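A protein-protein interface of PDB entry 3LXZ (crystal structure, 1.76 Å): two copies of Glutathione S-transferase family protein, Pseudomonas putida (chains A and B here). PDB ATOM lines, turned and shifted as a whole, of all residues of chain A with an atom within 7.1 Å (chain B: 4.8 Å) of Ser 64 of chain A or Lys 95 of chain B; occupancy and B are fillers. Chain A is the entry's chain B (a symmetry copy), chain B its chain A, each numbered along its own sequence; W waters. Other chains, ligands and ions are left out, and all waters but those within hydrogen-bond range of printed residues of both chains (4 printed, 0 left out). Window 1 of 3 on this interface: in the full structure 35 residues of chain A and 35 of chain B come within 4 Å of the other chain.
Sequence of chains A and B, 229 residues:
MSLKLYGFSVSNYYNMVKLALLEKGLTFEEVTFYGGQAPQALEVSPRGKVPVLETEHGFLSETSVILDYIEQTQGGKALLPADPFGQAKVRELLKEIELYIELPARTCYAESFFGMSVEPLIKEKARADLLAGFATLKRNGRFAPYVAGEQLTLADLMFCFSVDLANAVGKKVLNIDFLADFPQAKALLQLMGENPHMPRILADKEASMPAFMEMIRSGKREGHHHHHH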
ATOM      1  N   TYR A  13      -1.913  -0.029 -26.729  1.00  0.00           N
ATOM      2  CA  TYR A  13      -3.278   0.478 -26.508  1.00  0.00           C
ATOM      3  C   TYR A  13      -3.302   1.605 -25.446  1.00  0.00           C
ATOM      4  O   TYR A  13      -4.037   2.594 -25.567  1.00  0.00           O
ATOM      5  CB  TYR A  13      -4.246  -0.640 -26.088  1.00  0.00           C
ATOM      6  CG  TYR A  13      -4.654  -1.556 -27.244  1.00  0.00           C
ATOM      7  CD1 TYR A  13      -5.682  -1.198 -28.106  1.00  0.00           C
ATOM      8  CD2 TYR A  13      -4.018  -2.770 -27.451  1.00  0.00           C
ATOM      9  CE1 TYR A  13      -6.071  -2.024 -29.144  1.00  0.00           C
ATOM     10  CE2 TYR A  13      -4.414  -3.610 -28.508  1.00  0.00           C
ATOM     11  CZ  TYR A  13      -5.420  -3.223 -29.326  1.00  0.00           C
ATOM     12  OH  TYR A  13      -5.744  -4.081 -30.315  1.00  0.00           O
ATOM     13  N   MET A  16      -1.982   4.827 -27.045  1.00  0.00           N
ATOM     14  CA  MET A  16      -2.950   5.518 -27.905  1.00  0.00           C
ATOM     15  C   MET A  16      -3.793   6.472 -27.067  1.00  0.00           C
ATOM     16  O   MET A  16      -4.032   7.605 -27.497  1.00  0.00           O
ATOM     17  CB  MET A  16      -3.882   4.527 -28.646  1.00  0.00           C
ATOM     18  CG  MET A  16      -3.108   3.523 -29.482  1.00  0.00           C
ATOM     19  SD  MET A  16      -4.351   2.168 -30.101  1.00  0.00           S
ATOM     20  CE  MET A  16      -3.037   0.819 -30.629  1.00  0.00           C
ATOM     21  N   VAL A  17      -4.293   6.012 -25.905  1.00  0.00           N
ATOM     22  CA  VAL A  17      -5.129   6.895 -25.077  1.00  0.00           C
ATOM     23  C   VAL A  17      -4.264   7.990 -24.424  1.00  0.00           C
ATOM     24  O   VAL A  17      -4.674   9.150 -24.344  1.00  0.00           O
ATOM     25  CB  VAL A  17      -5.967   6.144 -24.003  1.00  0.00           C
ATOM     26  CG1 VAL A  17      -6.839   7.139 -23.251  1.00  0.00           C
ATOM     27  CG2 VAL A  17      -6.852   5.048 -24.636  1.00  0.00           C
ATOM     28  N   PRO A  51      -5.814  -0.425 -21.911  1.00  0.00           N
ATOM     29  CA  PRO A  51      -5.918   0.283 -20.673  1.00  0.00           C
ATOM     30  C   PRO A  51      -7.353   0.326 -20.111  1.00  0.00           C
ATOM     31  O   PRO A  51      -8.298  -0.178 -20.692  1.00  0.00           O
ATOM     32  CB  PRO A  51      -5.482   1.701 -21.073  1.00  0.00           C
ATOM     33  CG  PRO A  51      -6.050   1.848 -22.451  1.00  0.00           C
ATOM     34  CD  PRO A  51      -6.010   0.487 -23.066  1.00  0.00           C
ATOM     35  N   SER A  61     -13.055   0.170 -20.013  1.00  0.00           N
ATOM     36  CA  SER A  61     -11.959  -0.542 -20.677  1.00  0.00           C
ATOM     37  C   SER A  61     -12.140  -0.444 -22.213  1.00  0.00           C
ATOM     38  O   SER A  61     -13.138   0.102 -22.694  1.00  0.00           O
ATOM     39  CB  SER A  61     -11.874  -2.031 -20.244  1.00  0.00           C
ATOM     40  OG  SER A  61     -13.006  -2.779 -20.704  1.00  0.00           O
ATOM     41  N   GLU A  62     -11.154  -0.963 -22.960  1.00  0.00           N
ATOM     42  CA  GLU A  62     -11.134  -0.960 -24.435  1.00  0.00           C
ATOM     43  C   GLU A  62     -10.781   0.428 -24.984  1.00  0.00           C
ATOM     44  O   GLU A  62     -11.582   1.349 -24.916  1.00  0.00           O
ATOM     45  CB  GLU A  62     -12.455  -1.493 -25.051  1.00  0.00           C
ATOM     46  CG  GLU A  62     -12.836  -2.919 -24.604  1.00  0.00           C
ATOM     47  CD  GLU A  62     -11.903  -4.024 -25.110  1.00  0.00           C
ATOM     48  OE1 GLU A  62     -11.223  -3.882 -26.156  1.00  0.00           O
ATOM     49  OE2 GLU A  62     -11.846  -5.080 -24.459  1.00  0.00           O
ATOM     50  N   THR A  63      -9.561   0.569 -25.493  1.00  0.00           N
ATOM     51  CA  THR A  63      -9.129   1.788 -26.166  1.00  0.00           C
ATOM     52  C   THR A  63     -10.178   2.460 -27.035  1.00  0.00           C
ATOM     53  O   THR A  63     -10.413   3.674 -26.884  1.00  0.00           O
ATOM     54  CB  THR A  63      -7.886   1.543 -26.978  1.00  0.00           C
ATOM     55  OG1 THR A  63      -6.838   1.259 -26.070  1.00  0.00           O
ATOM     56  CG2 THR A  63      -7.514   2.770 -27.740  1.00  0.00           C
ATOM     57  N   SER A  64     -10.834   1.703 -27.925  1.00  0.00           N
ATOM     58  CA  SER A  64     -11.766   2.332 -28.888  1.00  0.00           C
ATOM     59  C   SER A  64     -12.928   2.999 -28.118  1.00  0.00           C
ATOM     60  O   SER A  64     -13.385   4.118 -28.442  1.00  0.00           O
ATOM     61  CB  SER A  64     -12.280   1.274 -29.881  1.00  0.00           C
ATOM     62  OG  SER A  64     -13.005   0.259 -29.210  1.00  0.00           O
ATOM     63  N   VAL A  65     -13.349   2.341 -27.049  1.00  0.00           N
ATOM     64  CA  VAL A  65     -14.471   2.788 -26.201  1.00  0.00           C
ATOM     65  C   VAL A  65     -14.071   4.020 -25.372  1.00  0.00           C
ATOM     66  O   VAL A  65     -14.811   5.000 -25.285  1.00  0.00           O
ATOM     67  CB  VAL A  65     -14.911   1.642 -25.263  1.00  0.00           C
ATOM     68  CG1 VAL A  65     -16.001   2.121 -24.272  1.00  0.00           C
ATOM     69  CG2 VAL A  65     -15.527   0.463 -26.102  1.00  0.00           C
ATOM     70  N   ILE A  66     -12.868   3.941 -24.798  1.00  0.00           N
ATOM     71  CA  ILE A  66     -12.256   5.037 -24.033  1.00  0.00           C
ATOM     72  C   ILE A  66     -12.080   6.282 -24.892  1.00  0.00           C
ATOM     73  O   ILE A  66     -12.500   7.391 -24.486  1.00  0.00           O
ATOM     74  CB  ILE A  66     -10.946   4.612 -23.343  1.00  0.00           C
ATOM     75  CG1 ILE A  66     -11.259   3.550 -22.275  1.00  0.00           C
ATOM     76  CG2 ILE A  66     -10.266   5.800 -22.674  1.00  0.00           C
ATOM     77  CD1 ILE A  66     -10.024   2.677 -21.924  1.00  0.00           C
ATOM     78  N   LEU A  67     -11.527   6.108 -26.095  1.00  0.00           N
ATOM     79  CA  LEU A  67     -11.328   7.269 -26.997  1.00  0.00           C
ATOM     80  C   LEU A  67     -12.633   7.968 -27.350  1.00  0.00           C
ATOM     81  O   LEU A  67     -12.697   9.199 -27.360  1.00  0.00           O
ATOM     82  CB  LEU A  67     -10.559   6.887 -28.269  1.00  0.00           C
ATOM     83  CG  LEU A  67      -9.099   6.470 -28.066  1.00  0.00           C
ATOM     84  CD1 LEU A  67      -8.567   5.951 -29.395  1.00  0.00           C
ATOM     85  CD2 LEU A  67      -8.285   7.670 -27.545  1.00  0.00           C
ATOM     86  N   ASP A  68     -13.667   7.187 -27.646  1.00  0.00           N
ATOM     87  CA  ASP A  68     -14.983   7.743 -27.930  1.00  0.00           C
ATOM     88  C   ASP A  68     -15.567   8.499 -26.755  1.00  0.00           C
ATOM     89  O   ASP A  68     -16.180   9.561 -26.944  1.00  0.00           O
ATOM     90  CB  ASP A  68     -15.936   6.625 -28.368  1.00  0.00           C
ATOM     91  CG  ASP A  68     -15.795   6.280 -29.835  1.00  0.00           C
ATOM     92  OD1 ASP A  68     -15.044   6.946 -30.612  1.00  0.00           O
ATOM     93  OD2 ASP A  68     -16.491   5.352 -30.246  1.00  0.00           O
ATOM     94  N   TYR A  69     -15.394   7.952 -25.550  1.00  0.00           N
ATOM     95  CA  TYR A  69     -15.894   8.587 -24.332  1.00  0.00           C
ATOM     96  C   TYR A  69     -15.183   9.927 -24.121  1.00  0.00           C
ATOM     97  O   TYR A  69     -15.834  10.954 -23.812  1.00  0.00           O
ATOM     98  CB  TYR A  69     -15.705   7.655 -23.101  1.00  0.00           C
ATOM     99  CG  TYR A  69     -16.095   8.329 -21.805  1.00  0.00           C
ATOM    100  CD1 TYR A  69     -17.428   8.368 -21.387  1.00  0.00           C
ATOM    101  CD2 TYR A  69     -15.133   8.969 -21.015  1.00  0.00           C
ATOM    102  CE1 TYR A  69     -17.786   8.996 -20.191  1.00  0.00           C
ATOM    103  CE2 TYR A  69     -15.494   9.624 -19.836  1.00  0.00           C
ATOM    104  CZ  TYR A  69     -16.825   9.633 -19.435  1.00  0.00           C
ATOM    105  OH  TYR A  69     -17.173  10.288 -18.268  1.00  0.00           O
ATOM    106  N   ARG A  91     -14.181   5.940 -37.421  1.00  0.00           N
ATOM    107  CA  ARG A  91     -14.314   4.753 -36.592  1.00  0.00           C
ATOM    108  C   ARG A  91     -14.188   3.439 -37.373  1.00  0.00           C
ATOM    109  O   ARG A  91     -13.717   2.451 -36.826  1.00  0.00           O
ATOM    110  CB  ARG A  91     -15.619   4.843 -35.799  1.00  0.00           C
ATOM    111  CG  ARG A  91     -15.531   5.932 -34.721  1.00  0.00           C
ATOM    112  CD  ARG A  91     -16.910   6.406 -34.256  1.00  0.00           C
ATOM    113  NE  ARG A  91     -16.768   7.258 -33.076  1.00  0.00           N
ATOM    114  CZ  ARG A  91     -17.524   8.334 -32.838  1.00  0.00           C
ATOM    115  NH1 ARG A  91     -18.437   8.710 -33.727  1.00  0.00           N
ATOM    116  NH2 ARG A  91     -17.315   9.056 -31.743  1.00  0.00           N
ATOM    117  N   LEU A  94     -10.472   3.070 -37.831  1.00  0.00           N
ATOM    118  CA  LEU A  94      -9.904   2.635 -36.547  1.00  0.00           C
ATOM    119  C   LEU A  94     -10.189   1.144 -36.284  1.00  0.00           C
ATOM    120  O   LEU A  94      -9.254   0.360 -35.887  1.00  0.00           O
ATOM    121  CB  LEU A  94     -10.429   3.528 -35.400  1.00  0.00           C
ATOM    122  CG  LEU A  94      -9.789   3.254 -34.039  1.00  0.00           C
ATOM    123  CD1 LEU A  94      -9.864   4.523 -33.171  1.00  0.00           C
ATOM    124  CD2 LEU A  94     -10.486   2.110 -33.307  1.00  0.00           C
ATOM    125  N   LYS A  95     -11.459   0.742 -36.475  1.00  0.00           N
ATOM    126  CA  LYS A  95     -11.845  -0.667 -36.266  1.00  0.00           C
ATOM    127  C   LYS A  95     -11.051  -1.558 -37.197  1.00  0.00           C
ATOM    128  O   LYS A  95     -10.581  -2.657 -36.805  1.00  0.00           O
ATOM    129  CB  LYS A  95     -13.340  -0.891 -36.517  1.00  0.00           C
ATOM    130  CG  LYS A  95     -13.875  -2.233 -36.024  1.00  0.00           C
ATOM    131  CD  LYS A  95     -15.389  -2.249 -36.022  1.00  0.00           C
ATOM    132  CE  LYS A  95     -15.996  -3.606 -35.507  1.00  0.00           C
ATOM    133  NZ  LYS A  95     -15.311  -4.058 -34.270  1.00  0.00           N
ATOM    134  N   GLU A  98      -7.572  -1.967 -35.970  1.00  0.00           N
ATOM    135  CA  GLU A  98      -7.548  -2.817 -34.759  1.00  0.00           C
ATOM    136  C   GLU A  98      -7.737  -4.324 -35.076  1.00  0.00           C
ATOM    137  O   GLU A  98      -6.898  -5.171 -34.732  1.00  0.00           O
ATOM    138  CB  GLU A  98      -8.623  -2.320 -33.783  1.00  0.00           C
ATOM    139  CG  GLU A  98      -8.625  -3.066 -32.474  1.00  0.00           C
ATOM    140  CD  GLU A  98      -9.637  -2.552 -31.457  1.00  0.00           C
ATOM    141  OE1 GLU A  98      -9.897  -3.299 -30.486  1.00  0.00           O
ATOM    142  OE2 GLU A  98     -10.149  -1.422 -31.618  1.00  0.00           O
ATOM    143  N   LEU A  99      -8.851  -4.642 -35.735  1.00  0.00           N
ATOM    144  CA  LEU A  99      -9.203  -6.024 -36.015  1.00  0.00           C
ATOM    145  C   LEU A  99      -8.336  -6.709 -37.064  1.00  0.00           C
ATOM    146  O   LEU A  99      -8.075  -7.901 -36.933  1.00  0.00           O
ATOM    147  CB  LEU A  99     -10.659  -6.094 -36.447  1.00  0.00           C
ATOM    148  CG  LEU A  99     -11.670  -6.145 -35.293  1.00  0.00           C
ATOM    149  CD1 LEU A  99     -11.486  -4.996 -34.320  1.00  0.00           C
ATOM    150  CD2 LEU A  99     -13.129  -6.155 -35.850  1.00  0.00           C
ATOM    151  N   LEU A 154      -8.780  10.183 -34.351  1.00  0.00           N
ATOM    152  CA  LEU A 154      -8.557   8.946 -33.562  1.00  0.00           C
ATOM    153  C   LEU A 154      -7.924   7.806 -34.382  1.00  0.00           C
ATOM    154  O   LEU A 154      -7.151   6.969 -33.839  1.00  0.00           O
ATOM    155  CB  LEU A 154      -9.897   8.442 -32.982  1.00  0.00           C
ATOM    156  CG  LEU A 154     -10.619   9.397 -32.041  1.00  0.00           C
ATOM    157  CD1 LEU A 154     -11.931   8.747 -31.551  1.00  0.00           C
ATOM    158  CD2 LEU A 154      -9.721   9.802 -30.856  1.00  0.00           C
ATOM    159  N   MET A 158      -4.615   4.824 -33.535  1.00  0.00           N
ATOM    160  CA  MET A 158      -4.606   3.379 -33.732  1.00  0.00           C
ATOM    161  C   MET A 158      -3.558   3.024 -34.784  1.00  0.00           C
ATOM    162  O   MET A 158      -2.836   2.030 -34.636  1.00  0.00           O
ATOM    163  CB  MET A 158      -6.031   2.881 -34.119  1.00  0.00           C
ATOM    164  CG  MET A 158      -6.180   1.397 -34.362  1.00  0.00           C
ATOM    165  SD  MET A 158      -5.920   0.271 -32.801  1.00  0.00           S
ATOM    166  CE  MET A 158      -7.471   0.815 -31.726  1.00  0.00           C
ATOM    167  N   ARG B  91     -21.307   0.388 -25.284  1.00  0.00           N
ATOM    168  CA  ARG B  91     -20.287   0.116 -26.306  1.00  0.00           C
ATOM    169  C   ARG B  91     -19.171  -0.811 -25.849  1.00  0.00           C
ATOM    170  O   ARG B  91     -18.689  -1.635 -26.640  1.00  0.00           O
ATOM    171  CB  ARG B  91     -19.740   1.411 -26.874  1.00  0.00           C
ATOM    172  CG  ARG B  91     -20.808   2.122 -27.715  1.00  0.00           C
ATOM    173  CD  ARG B  91     -20.443   3.543 -28.065  1.00  0.00           C
ATOM    174  NE  ARG B  91     -21.405   4.093 -28.999  1.00  0.00           N
ATOM    175  CZ  ARG B  91     -22.046   5.255 -28.848  1.00  0.00           C
ATOM    176  NH1 ARG B  91     -21.828   6.027 -27.800  1.00  0.00           N
ATOM    177  NH2 ARG B  91     -22.917   5.638 -29.767  1.00  0.00           N
ATOM    178  N   GLU B  92     -18.744  -0.662 -24.593  1.00  0.00           N
ATOM    179  CA  GLU B  92     -17.807  -1.631 -23.962  1.00  0.00           C
ATOM    180  C   GLU B  92     -18.363  -3.068 -23.979  1.00  0.00           C
ATOM    181  O   GLU B  92     -17.700  -4.016 -24.426  1.00  0.00           O
ATOM    182  CB  GLU B  92     -17.436  -1.190 -22.546  1.00  0.00           C
ATOM    183  CG  GLU B  92     -16.412  -2.075 -21.851  1.00  0.00           C
ATOM    184  CD  GLU B  92     -16.397  -1.852 -20.344  1.00  0.00           C
ATOM    185  OE1 GLU B  92     -17.496  -1.732 -19.728  1.00  0.00           O
ATOM    186  OE2 GLU B  92     -15.280  -1.800 -19.762  1.00  0.00           O
ATOM    187  N   LEU B  93     -19.585  -3.242 -23.489  1.00  0.00           N
ATOM    188  CA  LEU B  93     -20.223  -4.549 -23.567  1.00  0.00           C
ATOM    189  C   LEU B  93     -20.398  -5.111 -24.993  1.00  0.00           C
ATOM    190  O   LEU B  93     -20.107  -6.304 -25.251  1.00  0.00           O
ATOM    191  CB  LEU B  93     -21.585  -4.491 -22.832  1.00  0.00           C
ATOM    192  CG  LEU B  93     -21.420  -4.448 -21.300  1.00  0.00           C
ATOM    193  CD1 LEU B  93     -22.703  -3.913 -20.619  1.00  0.00           C
ATOM    194  CD2 LEU B  93     -21.058  -5.806 -20.698  1.00  0.00           C
ATOM    195  N   LEU B  94     -20.859  -4.274 -25.923  1.00  0.00           N
ATOM    196  CA  LEU B  94     -20.964  -4.698 -27.320  1.00  0.00           C
ATOM    197  C   LEU B  94     -19.596  -5.175 -27.859  1.00  0.00           C
ATOM    198  O   LEU B  94     -19.499  -6.242 -28.485  1.00  0.00           O
ATOM    199  CB  LEU B  94     -21.509  -3.571 -28.207  1.00  0.00           C
ATOM    200  CG  LEU B  94     -21.810  -3.926 -29.683  1.00  0.00           C
ATOM    201  CD1 LEU B  94     -22.821  -2.913 -30.173  1.00  0.00           C
ATOM    202  CD2 LEU B  94     -20.548  -3.837 -30.606  1.00  0.00           C
ATOM    203  N   LYS B  95     -18.554  -4.392 -27.601  1.00  0.00           N
ATOM    204  CA  LYS B  95     -17.190  -4.744 -28.038  1.00  0.00           C
ATOM    205  C   LYS B  95     -16.710  -6.059 -27.423  1.00  0.00           C
ATOM    206  O   LYS B  95     -16.059  -6.886 -28.112  1.00  0.00           O
ATOM    207  CB  LYS B  95     -16.179  -3.661 -27.654  1.00  0.00           C
ATOM    208  CG  LYS B  95     -14.848  -3.801 -28.394  1.00  0.00           C
ATOM    209  CD  LYS B  95     -13.923  -2.647 -28.112  1.00  0.00           C
ATOM    210  CE  LYS B  95     -12.533  -2.851 -28.842  1.00  0.00           C
ATOM    211  NZ  LYS B  95     -12.651  -2.354 -30.235  1.00  0.00           N
ATOM    212  N   GLU B  96     -16.981  -6.242 -26.140  1.00  0.00           N
ATOM    213  CA  GLU B  96     -16.564  -7.474 -25.470  1.00  0.00           C
ATOM    214  C   GLU B  96     -17.245  -8.690 -26.076  1.00  0.00           C
ATOM    215  O   GLU B  96     -16.638  -9.752 -26.220  1.00  0.00           O
ATOM    216  CB  GLU B  96     -16.833  -7.435 -23.960  1.00  0.00           C
ATOM    217  CG  GLU B  96     -15.881  -6.487 -23.255  1.00  0.00           C
ATOM    218  CD  GLU B  96     -16.287  -6.039 -21.860  1.00  0.00           C
ATOM    219  OE1 GLU B  96     -17.467  -6.192 -21.386  1.00  0.00           O
ATOM    220  OE2 GLU B  96     -15.356  -5.498 -21.232  1.00  0.00           O
ATOM    221  N   ILE B  97     -18.530  -8.569 -26.375  1.00  0.00           N
ATOM    222  CA  ILE B  97     -19.236  -9.703 -26.942  1.00  0.00           C
ATOM    223  C   ILE B  97     -18.663 -10.014 -28.318  1.00  0.00           C
ATOM    224  O   ILE B  97     -18.375 -11.163 -28.641  1.00  0.00           O
ATOM    225  CB  ILE B  97     -20.768  -9.498 -26.972  1.00  0.00           C
ATOM    226  CG1 ILE B  97     -21.323  -9.415 -25.560  1.00  0.00           C
ATOM    227  CG2 ILE B  97     -21.416 -10.675 -27.681  1.00  0.00           C
ATOM    228  CD1 ILE B  97     -22.732  -8.720 -25.518  1.00  0.00           C
ATOM    229  N   GLU B  98     -18.443  -8.979 -29.112  1.00  0.00           N
ATOM    230  CA  GLU B  98     -17.848  -9.155 -30.428  1.00  0.00           C
ATOM    231  C   GLU B  98     -16.471  -9.811 -30.366  1.00  0.00           C
ATOM    232  O   GLU B  98     -16.280 -10.844 -30.980  1.00  0.00           O
ATOM    233  CB  GLU B  98     -17.795  -7.827 -31.210  1.00  0.00           C
ATOM    234  CG  GLU B  98     -17.182  -7.951 -32.618  1.00  0.00           C
ATOM    235  CD  GLU B  98     -17.223  -6.643 -33.387  1.00  0.00           C
ATOM    236  OE1 GLU B  98     -17.926  -5.695 -32.945  1.00  0.00           O
ATOM    237  OE2 GLU B  98     -16.534  -6.560 -34.439  1.00  0.00           O
ATOM    238  N   LEU B  99     -15.520  -9.217 -29.634  1.00  0.00           N
ATOM    239  CA  LEU B  99     -14.138  -9.685 -29.724  1.00  0.00           C
ATOM    240  C   LEU B  99     -13.941 -10.965 -28.918  1.00  0.00           C
ATOM    241  O   LEU B  99     -13.056 -11.758 -29.240  1.00  0.00           O
ATOM    242  CB  LEU B  99     -13.179  -8.625 -29.145  1.00  0.00           C
ATOM    243  CG  LEU B  99     -12.659  -7.547 -30.112  1.00  0.00           C
ATOM    244  CD1 LEU B  99     -13.780  -6.843 -30.748  1.00  0.00           C
ATOM    245  CD2 LEU B  99     -11.692  -6.551 -29.444  1.00  0.00           C
ATOM    246  N   TYR B 100     -14.731 -11.161 -27.869  1.00  0.00           N
ATOM    247  CA  TYR B 100     -14.393 -12.238 -26.930  1.00  0.00           C
ATOM    248  C   TYR B 100     -15.377 -13.373 -26.931  1.00  0.00           C
ATOM    249  O   TYR B 100     -15.128 -14.418 -26.285  1.00  0.00           O
ATOM    250  CB  TYR B 100     -14.160 -11.714 -25.493  1.00  0.00           C
ATOM    251  CG  TYR B 100     -13.213 -10.540 -25.492  1.00  0.00           C
ATOM    252  CD1 TYR B 100     -11.971 -10.635 -26.123  1.00  0.00           C
ATOM    253  CD2 TYR B 100     -13.592  -9.337 -24.931  1.00  0.00           C
ATOM    254  CE1 TYR B 100     -11.099  -9.530 -26.178  1.00  0.00           C
ATOM    255  CE2 TYR B 100     -12.753  -8.232 -24.965  1.00  0.00           C
ATOM    256  CZ  TYR B 100     -11.508  -8.338 -25.596  1.00  0.00           C
ATOM    257  OH  TYR B 100     -10.704  -7.222 -25.607  1.00  0.00           O
HETATM  258  O   HOH W   1     -12.941  -0.641 -32.636  1.00  0.00           O
HETATM  259  O   HOH W   2     -17.032  -3.380 -31.419  1.00  0.00           O
HETATM  260  O   HOH W   3     -12.909  -5.019 -21.976  1.00  0.00           O
HETATM  261  O   HOH W   4     -19.215   5.995 -30.882  1.00  0.00           O
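Ser 61 of chain A touches Glu 96 of chain B. CE of Lys 95 of chain B touches OE1 of Glu 62 of chain A, at 3.2 Å. CG2 of Val 65 of chain A touches O of Arg 91 of chain B, at 3.8 Å. Glu 92 of chain B touches Val 65 of chain A. OE1 of Glu 98 of chain A touches CD2 of Leu 99 of chain B, at 3.9 Å. CD2 of Leu 99 of chain A touches OE2 of Glu 98 of chain B (3.7 Å).
OG of Ser 61 of chain A sits at hydrogen-bond distance from OE2 of Glu 92 of chain B, 2.6 Å away. OG of Ser 64 of chain A is in hydrogen-bond range of NZ of Lys 95 of chain B. The side-chain carboxylate (OE1) of Glu 98 of chain A lies within salt-bridge range of the side-chain amino group (NZ) of Lys 95 of chain B (2.9 Å). OE2 of Glu 98 of chain B lies within salt-bridge range of NZ of Lys 95 of chain A (2.8 Å). The side-chain hydroxyl of Tyr 100 of chain B lies within hydrogen-bond range of the side-chain carboxylate of Glu 62 of chain A (2.7 Å).
Water W3 lies within hydrogen-bond range of OG of Ser 61 of chain A, OE2 of Glu 96 of chain B and OE2 of Glu 62 of chain A. Water W4 lies within hydrogen-bond range of the side-chain carboxylate (OD2) of Asp 68 of chain A (2.9 Å) and the guanidinium group (NE) of Arg 91 of chain B (3.5 Å). Water W2 bridges the side-chain carboxylate of Glu 98 of chain B (2.9 Å) and the side-chain amino group of Lys 95 of chain A (3.4 Å). Water W1 lies within hydrogen-bond range of the side-chain amino group of Lys 95 of chain B and the side-chain carboxylate of Glu 98 of chain A.
Of the printed residues of chain B, Glu 98 of chain A touches Lys 95 and Leu 99. Of the printed residues of chain A, Arg 91 of chain B touches Val 65 (3.8 Å). Printed residues of chain A within 4 Å of Glu 96 of chain B: Ser 61 (3.6 Å). Of the printed residues of chain A, Tyr 100 of chain B touches Glu 62. The nearest residue of chain A that does not touch Lys 95 of chain B is Val 65 of chain A (4.04 Å). The nearest printed residue of chain A that does not touch Arg 91 of chain B is Asp 68 of chain A (4.9 Å).
Lys 95 of chain A touches Glu 98 of chain B, and with the chains exchanged Glu 98 of chain A touches Lys 95 of chain B. Glu 98 of chain A touches Leu 99 of chain B, and with the chains exchanged Leu 99 of chain A touches Glu 98 of chain B. Positions printed for both chains: 91, 94, 95, 98 and 99.
Of the 10 printed residues of chain B, 7 touch a printed residue of chain A. Printed residues of chain B that touch a printed residue of chain A: Arg 91, Glu 92, Lys 95, Glu 96, Glu 98, Leu 99 and Tyr 100. Of the 20 printed residues of chain A, 7 touch a printed residue of chain B. Hydrophobic or aromatic side chains of chain A that line the printed part of chain B: Val 65 and Leu 99. Among the printed residues, Asp or Glu carboxylates within 4 Å of a Lys or Arg side-chain nitrogen of the other chain: Lys 95 of chain A with Glu 98 of chain B (2.8 Å) and Glu 98 of chain A with Lys 95 of chain B (2.9 Å).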
